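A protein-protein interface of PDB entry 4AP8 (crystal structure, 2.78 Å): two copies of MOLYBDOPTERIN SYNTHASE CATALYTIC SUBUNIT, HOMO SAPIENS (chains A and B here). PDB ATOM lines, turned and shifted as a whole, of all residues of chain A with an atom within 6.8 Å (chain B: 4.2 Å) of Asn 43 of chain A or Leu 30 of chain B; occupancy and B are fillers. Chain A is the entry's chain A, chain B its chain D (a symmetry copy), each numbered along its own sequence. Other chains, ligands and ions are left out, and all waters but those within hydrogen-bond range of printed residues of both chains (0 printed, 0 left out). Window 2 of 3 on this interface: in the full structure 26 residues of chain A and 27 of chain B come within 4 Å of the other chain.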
ATOM      1  N   THR A  40     -17.388   2.957 -30.651  1.00  0.00           N
ATOM      2  CA  THR A  40     -16.539   1.919 -31.247  1.00  0.00           C
ATOM      3  C   THR A  40     -17.264   0.600 -31.160  1.00  0.00           C
ATOM      4  O   THR A  40     -18.137   0.436 -30.328  1.00  0.00           O
ATOM      5  CB  THR A  40     -15.103   1.818 -30.619  1.00  0.00           C
ATOM      6  OG1 THR A  40     -15.123   1.509 -29.206  1.00  0.00           O
ATOM      7  CG2 THR A  40     -14.405   3.093 -30.796  1.00  0.00           C
ATOM      8  N   THR A  41     -16.912  -0.321 -32.056  1.00  0.00           N
ATOM      9  CA  THR A  41     -17.463  -1.660 -32.048  1.00  0.00           C
ATOM     10  C   THR A  41     -16.784  -2.460 -30.971  1.00  0.00           C
ATOM     11  O   THR A  41     -15.578  -2.735 -31.025  1.00  0.00           O
ATOM     12  CB  THR A  41     -17.278  -2.358 -33.408  1.00  0.00           C
ATOM     13  OG1 THR A  41     -18.081  -1.696 -34.395  1.00  0.00           O
ATOM     14  CG2 THR A  41     -17.710  -3.796 -33.318  1.00  0.00           C
ATOM     15  N   ARG A  42     -17.568  -2.844 -29.976  1.00  0.00           N
ATOM     16  CA  ARG A  42     -17.048  -3.679 -28.914  1.00  0.00           C
ATOM     17  C   ARG A  42     -17.058  -5.142 -29.377  1.00  0.00           C
ATOM     18  O   ARG A  42     -17.922  -5.556 -30.161  1.00  0.00           O
ATOM     19  CB  ARG A  42     -17.891  -3.491 -27.665  1.00  0.00           C
ATOM     20  CG  ARG A  42     -17.291  -4.044 -26.380  1.00  0.00           C
ATOM     21  CD  ARG A  42     -18.233  -3.838 -25.203  1.00  0.00           C
ATOM     22  NE  ARG A  42     -19.194  -2.814 -25.576  1.00  0.00           N
ATOM     23  CZ  ARG A  42     -20.496  -3.015 -25.736  1.00  0.00           C
ATOM     24  NH1 ARG A  42     -20.991  -4.209 -25.478  1.00  0.00           N
ATOM     25  NH2 ARG A  42     -21.296  -1.995 -26.135  1.00  0.00           N
ATOM     26  N   ASN A  43     -16.099  -5.921 -28.877  1.00  0.00           N
ATOM     27  CA  ASN A  43     -15.883  -7.301 -29.324  1.00  0.00           C
ATOM     28  C   ASN A  43     -16.756  -8.356 -28.674  1.00  0.00           C
ATOM     29  O   ASN A  43     -16.462  -9.549 -28.786  1.00  0.00           O
ATOM     30  CB  ASN A  43     -14.427  -7.700 -29.169  1.00  0.00           C
ATOM     31  CG  ASN A  43     -14.052  -8.048 -27.761  1.00  0.00           C
ATOM     32  OD1 ASN A  43     -14.893  -8.138 -26.839  1.00  0.00           O
ATOM     33  ND2 ASN A  43     -12.747  -8.257 -27.575  1.00  0.00           N
ATOM     34  N   ASN A  44     -17.857  -7.935 -28.059  1.00  0.00           N
ATOM     35  CA  ASN A  44     -18.815  -8.883 -27.506  1.00  0.00           C
ATOM     36  C   ASN A  44     -20.193  -8.287 -27.250  1.00  0.00           C
ATOM     37  O   ASN A  44     -20.331  -7.090 -27.036  1.00  0.00           O
ATOM     38  CB  ASN A  44     -18.278  -9.428 -26.197  1.00  0.00           C
ATOM     39  CG  ASN A  44     -17.962  -8.332 -25.199  1.00  0.00           C
ATOM     40  OD1 ASN A  44     -18.759  -8.073 -24.325  1.00  0.00           O
ATOM     41  ND2 ASN A  44     -16.808  -7.680 -25.338  1.00  0.00           N
ATOM     42  N   PHE A  45     -21.191  -9.158 -27.232  1.00  0.00           N
ATOM     43  CA  PHE A  45     -22.566  -8.786 -26.957  1.00  0.00           C
ATOM     44  C   PHE A  45     -23.224  -9.959 -26.274  1.00  0.00           C
ATOM     45  O   PHE A  45     -23.155 -11.092 -26.782  1.00  0.00           O
ATOM     46  CB  PHE A  45     -23.301  -8.462 -28.254  1.00  0.00           C
ATOM     47  CG  PHE A  45     -24.645  -7.816 -28.052  1.00  0.00           C
ATOM     48  CD1 PHE A  45     -24.763  -6.647 -27.302  1.00  0.00           C
ATOM     49  CD2 PHE A  45     -25.799  -8.365 -28.628  1.00  0.00           C
ATOM     50  CE1 PHE A  45     -25.997  -6.039 -27.119  1.00  0.00           C
ATOM     51  CE2 PHE A  45     -27.039  -7.756 -28.445  1.00  0.00           C
ATOM     52  CZ  PHE A  45     -27.135  -6.586 -27.697  1.00  0.00           C
ATOM     53  N   LYS A  48     -21.730 -13.731 -26.481  1.00  0.00           N
ATOM     54  CA  LYS A  48     -21.143 -14.198 -27.751  1.00  0.00           C
ATOM     55  C   LYS A  48     -20.081 -13.151 -28.287  1.00  0.00           C
ATOM     56  O   LYS A  48     -20.145 -11.971 -27.959  1.00  0.00           O
ATOM     57  CB  LYS A  48     -22.264 -14.638 -28.756  1.00  0.00           C
ATOM     58  N   LYS A  49     -19.046 -13.642 -28.982  1.00  0.00           N
ATOM     59  CA  LYS A  49     -17.964 -12.839 -29.582  1.00  0.00           C
ATOM     60  C   LYS A  49     -18.485 -12.113 -30.839  1.00  0.00           C
ATOM     61  O   LYS A  49     -19.047 -12.731 -31.745  1.00  0.00           O
ATOM     62  CB  LYS A  49     -16.758 -13.757 -29.941  1.00  0.00           C
ATOM     63  CG  LYS A  49     -15.484 -13.101 -30.516  1.00  0.00           C
ATOM     64  CD  LYS A  49     -14.508 -14.114 -31.185  1.00  0.00           C
ATOM     65  N   VAL A  50     -18.273 -10.799 -30.901  1.00  0.00           N
ATOM     66  CA  VAL A  50     -18.650 -10.002 -32.076  1.00  0.00           C
ATOM     67  C   VAL A  50     -17.417  -9.701 -32.920  1.00  0.00           C
ATOM     68  O   VAL A  50     -16.377  -9.323 -32.378  1.00  0.00           O
ATOM     69  CB  VAL A  50     -19.283  -8.653 -31.664  1.00  0.00           C
ATOM     70  CG1 VAL A  50     -19.578  -7.804 -32.889  1.00  0.00           C
ATOM     71  CG2 VAL A  50     -20.548  -8.843 -30.840  1.00  0.00           C
ATOM     72  N   ILE A  51     -17.524  -9.825 -34.240  1.00  0.00           N
ATOM     73  CA  ILE A  51     -16.409  -9.412 -35.125  1.00  0.00           C
ATOM     74  C   ILE A  51     -16.626  -8.077 -35.801  1.00  0.00           C
ATOM     75  O   ILE A  51     -15.654  -7.360 -36.065  1.00  0.00           O
ATOM     76  CB  ILE A  51     -16.023 -10.462 -36.186  1.00  0.00           C
ATOM     77  CG1 ILE A  51     -17.215 -10.872 -37.068  1.00  0.00           C
ATOM     78  CG2 ILE A  51     -15.415 -11.656 -35.463  1.00  0.00           C
ATOM     79  CD1 ILE A  51     -16.873 -11.878 -38.169  1.00  0.00           C
ATOM     80  N   VAL A  93     -14.483  -4.470 -35.141  1.00  0.00           N
ATOM     81  CA  VAL A  93     -14.063  -4.292 -33.741  1.00  0.00           C
ATOM     82  C   VAL A  93     -12.992  -3.215 -33.613  1.00  0.00           C
ATOM     83  O   VAL A  93     -12.115  -3.159 -34.434  1.00  0.00           O
ATOM     84  CB  VAL A  93     -13.438  -5.594 -33.180  1.00  0.00           C
ATOM     85  CG1 VAL A  93     -12.783  -5.331 -31.840  1.00  0.00           C
ATOM     86  CG2 VAL A  93     -14.477  -6.712 -33.053  1.00  0.00           C
ATOM     87  N   SER A  94     -13.120  -2.345 -32.618  1.00  0.00           N
ATOM     88  CA  SER A  94     -12.154  -1.285 -32.348  1.00  0.00           C
ATOM     89  C   SER A  94     -12.151  -0.131 -33.358  1.00  0.00           C
ATOM     90  O   SER A  94     -11.372   0.786 -33.218  1.00  0.00           O
ATOM     91  CB  SER A  94     -10.725  -1.858 -32.198  1.00  0.00           C
ATOM     92  OG  SER A  94     -10.537  -2.452 -30.921  1.00  0.00           O
ATOM     93  N   GLU B   4      -6.374  -7.808 -20.505  1.00  0.00           N
ATOM     94  CA  GLU B   4      -5.699  -6.524 -20.822  1.00  0.00           C
ATOM     95  C   GLU B   4      -5.609  -5.591 -19.587  1.00  0.00           C
ATOM     96  O   GLU B   4      -6.621  -5.061 -19.143  1.00  0.00           O
ATOM     97  CB  GLU B   4      -6.505  -5.854 -21.956  1.00  0.00           C
ATOM     98  CG  GLU B   4      -6.096  -4.449 -22.431  1.00  0.00           C
ATOM     99  CD  GLU B   4      -7.116  -3.806 -23.419  1.00  0.00           C
ATOM    100  OE1 GLU B   4      -8.252  -4.313 -23.604  1.00  0.00           O
ATOM    101  OE2 GLU B   4      -6.791  -2.780 -24.049  1.00  0.00           O
ATOM    102  N   SER B  28      -9.806   0.281 -26.783  1.00  0.00           N
ATOM    103  CA  SER B  28      -9.899  -1.123 -26.366  1.00  0.00           C
ATOM    104  C   SER B  28     -11.014  -1.883 -27.090  1.00  0.00           C
ATOM    105  O   SER B  28     -12.073  -1.328 -27.462  1.00  0.00           O
ATOM    106  CB  SER B  28     -10.094  -1.263 -24.852  1.00  0.00           C
ATOM    107  OG  SER B  28     -10.298  -2.619 -24.461  1.00  0.00           O
ATOM    108  N   PRO B  29     -10.758  -3.168 -27.330  1.00  0.00           N
ATOM    109  CA  PRO B  29     -11.753  -4.035 -27.920  1.00  0.00           C
ATOM    110  C   PRO B  29     -12.850  -4.330 -26.955  1.00  0.00           C
ATOM    111  O   PRO B  29     -13.885  -4.791 -27.383  1.00  0.00           O
ATOM    112  CB  PRO B  29     -10.985  -5.320 -28.205  1.00  0.00           C
ATOM    113  CG  PRO B  29      -9.577  -4.890 -28.315  1.00  0.00           C
ATOM    114  CD  PRO B  29      -9.445  -3.818 -27.282  1.00  0.00           C
ATOM    115  N   LEU B  30     -12.619  -4.084 -25.666  1.00  0.00           N
ATOM    116  CA  LEU B  30     -13.652  -4.304 -24.655  1.00  0.00           C
ATOM    117  C   LEU B  30     -14.467  -3.061 -24.464  1.00  0.00           C
ATOM    118  O   LEU B  30     -15.503  -3.117 -23.842  1.00  0.00           O
ATOM    119  CB  LEU B  30     -13.060  -4.753 -23.318  1.00  0.00           C
ATOM    120  CG  LEU B  30     -12.271  -6.072 -23.366  1.00  0.00           C
ATOM    121  CD1 LEU B  30     -11.475  -6.281 -22.088  1.00  0.00           C
ATOM    122  CD2 LEU B  30     -13.161  -7.280 -23.648  1.00  0.00           C
ATOM    123  N   CYS B  31     -14.079  -1.968 -25.097  1.00  0.00           N
ATOM    124  CA  CYS B  31     -14.856  -0.738 -25.006  1.00  0.00           C
ATOM    125  C   CYS B  31     -15.598  -0.358 -26.268  1.00  0.00           C
ATOM    126  O   CYS B  31     -15.069  -0.450 -27.404  1.00  0.00           O
ATOM    127  CB  CYS B  31     -13.923   0.389 -24.668  1.00  0.00           C
ATOM    128  SG  CYS B  31     -13.165   0.149 -23.071  1.00  0.00           S
ATOM    129  N   GLY B  32     -16.803   0.140 -26.026  1.00  0.00           N
ATOM    130  CA  GLY B  32     -17.664   0.712 -27.048  1.00  0.00           C
ATOM    131  C   GLY B  32     -17.774   2.234 -27.039  1.00  0.00           C
ATOM    132  O   GLY B  32     -18.393   2.816 -27.960  1.00  0.00           O
ATOM    133  N   ALA B 105     -17.099   0.286 -21.567  1.00  0.00           N
ATOM    134  CA  ALA B 105     -18.025  -0.609 -22.246  1.00  0.00           C
ATOM    135  C   ALA B 105     -19.142   0.210 -22.852  1.00  0.00           C
ATOM    136  O   ALA B 105     -19.431   0.109 -24.053  1.00  0.00           O
ATOM    137  CB  ALA B 105     -18.608  -1.600 -21.256  1.00  0.00           C
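The backbone NH (N) of Thr 40 of chain A is in hydrogen-bond range of the backbone carbonyl oxygen (O) of Gly 32 of chain B (2.9 Å).
NE of Arg 42 of chain A sits at hydrogen-bond distance from O of Ala 105 of chain B (3.3 Å).
The side-chain hydroxyl (OG1) of Thr 40 of chain A is in hydrogen-bond range of the backbone carbonyl oxygen (O) of Cys 31 of chain B (2.7 Å).
N of Asn 43 of chain A lies within hydrogen-bond range of O of Pro 29 of chain B (2.9 Å).
The side-chain carboxylate (OE1) of Glu 4 of chain B is in hydrogen-bond range of the side-chain hydroxyl (OG) of Ser 28 of chain B (2.8 Å).
The guanidinium group (NH1) of Arg 42 of chain A lies within hydrogen-bond range of the backbone carbonyl oxygen (O) of Asn 44 of chain A, 3.3 Å away.
The backbone NH (N) of Gly 32 of chain B lies within hydrogen-bond range of the backbone carbonyl oxygen (O) of Ala 105 of chain B (3.3 Å).
OD1 of Asn 43 of chain A lies within hydrogen-bond range of ND2 of Asn 44 of chain A, 2.5 Å away.
The side-chain hydroxyl (OG) of Ser 28 of chain B is in hydrogen-bond range of the backbone NH (N) of Leu 30 of chain B.
O of Thr 41 of chain A is in hydrogen-bond range of N of Ser 94 of chain A, at 3.0 Å.
Among the printed residues, pairs that only touch across the chains: Arg 42 of chain A with Leu 30 of chain B, Ser 94 of chain A with Pro 29 of chain B, Arg 42 of chain A with Pro 29 of chain B, Asn 43 of chain A with Leu 30 of chain B, Arg 42 of chain A with Gly 32 of chain B and Ser 94 of chain A with Ser 28 of chain B.
Of chain B, only Pro 29 and Leu 30 come within 4 Å of Asn 43 of chain A.
Printed residues of chain B within 4 Å of Ser 94 of chain A: Ser 28 and Pro 29.
Printed residues of chain A within 4 Å of Ser 28 of chain B: Ser 94 (3.9 Å).
Of the printed residues of chain A, Gly 32 of chain B touches Thr 40 (2.9 Å) and Arg 42 (3.8 Å).
Printed residues of chain A within 4 Å of Ala 105 of chain B: Arg 42 (3.3 Å).
The nearest printed residue of chain B that does not touch Asn 43 of chain A is Cys 31 of chain B (5.8 Å).
The nearest printed residue of chain A that does not touch Pro 29 of chain B is Val 93 of chain A (4.1 Å).
Of the 7 printed residues of chain B, 6 touch a printed residue of chain A.
Of the 12 printed residues of chain A, 4 touch a printed residue of chain B.
Along chain A the printed residues that touch a printed residue of chain B span positions 40 to 94.
Among the printed residues, 10 pairs touch across the chains.
Among the printed residues, no Asp or Glu carboxylate lies within 4 Å of a Lys or Arg side-chain nitrogen of the other chain.
No position is printed for both chains.
Of the 10 pairs that touch across the chains among the printed residues, none has its exchanged pair printed and touching as well.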
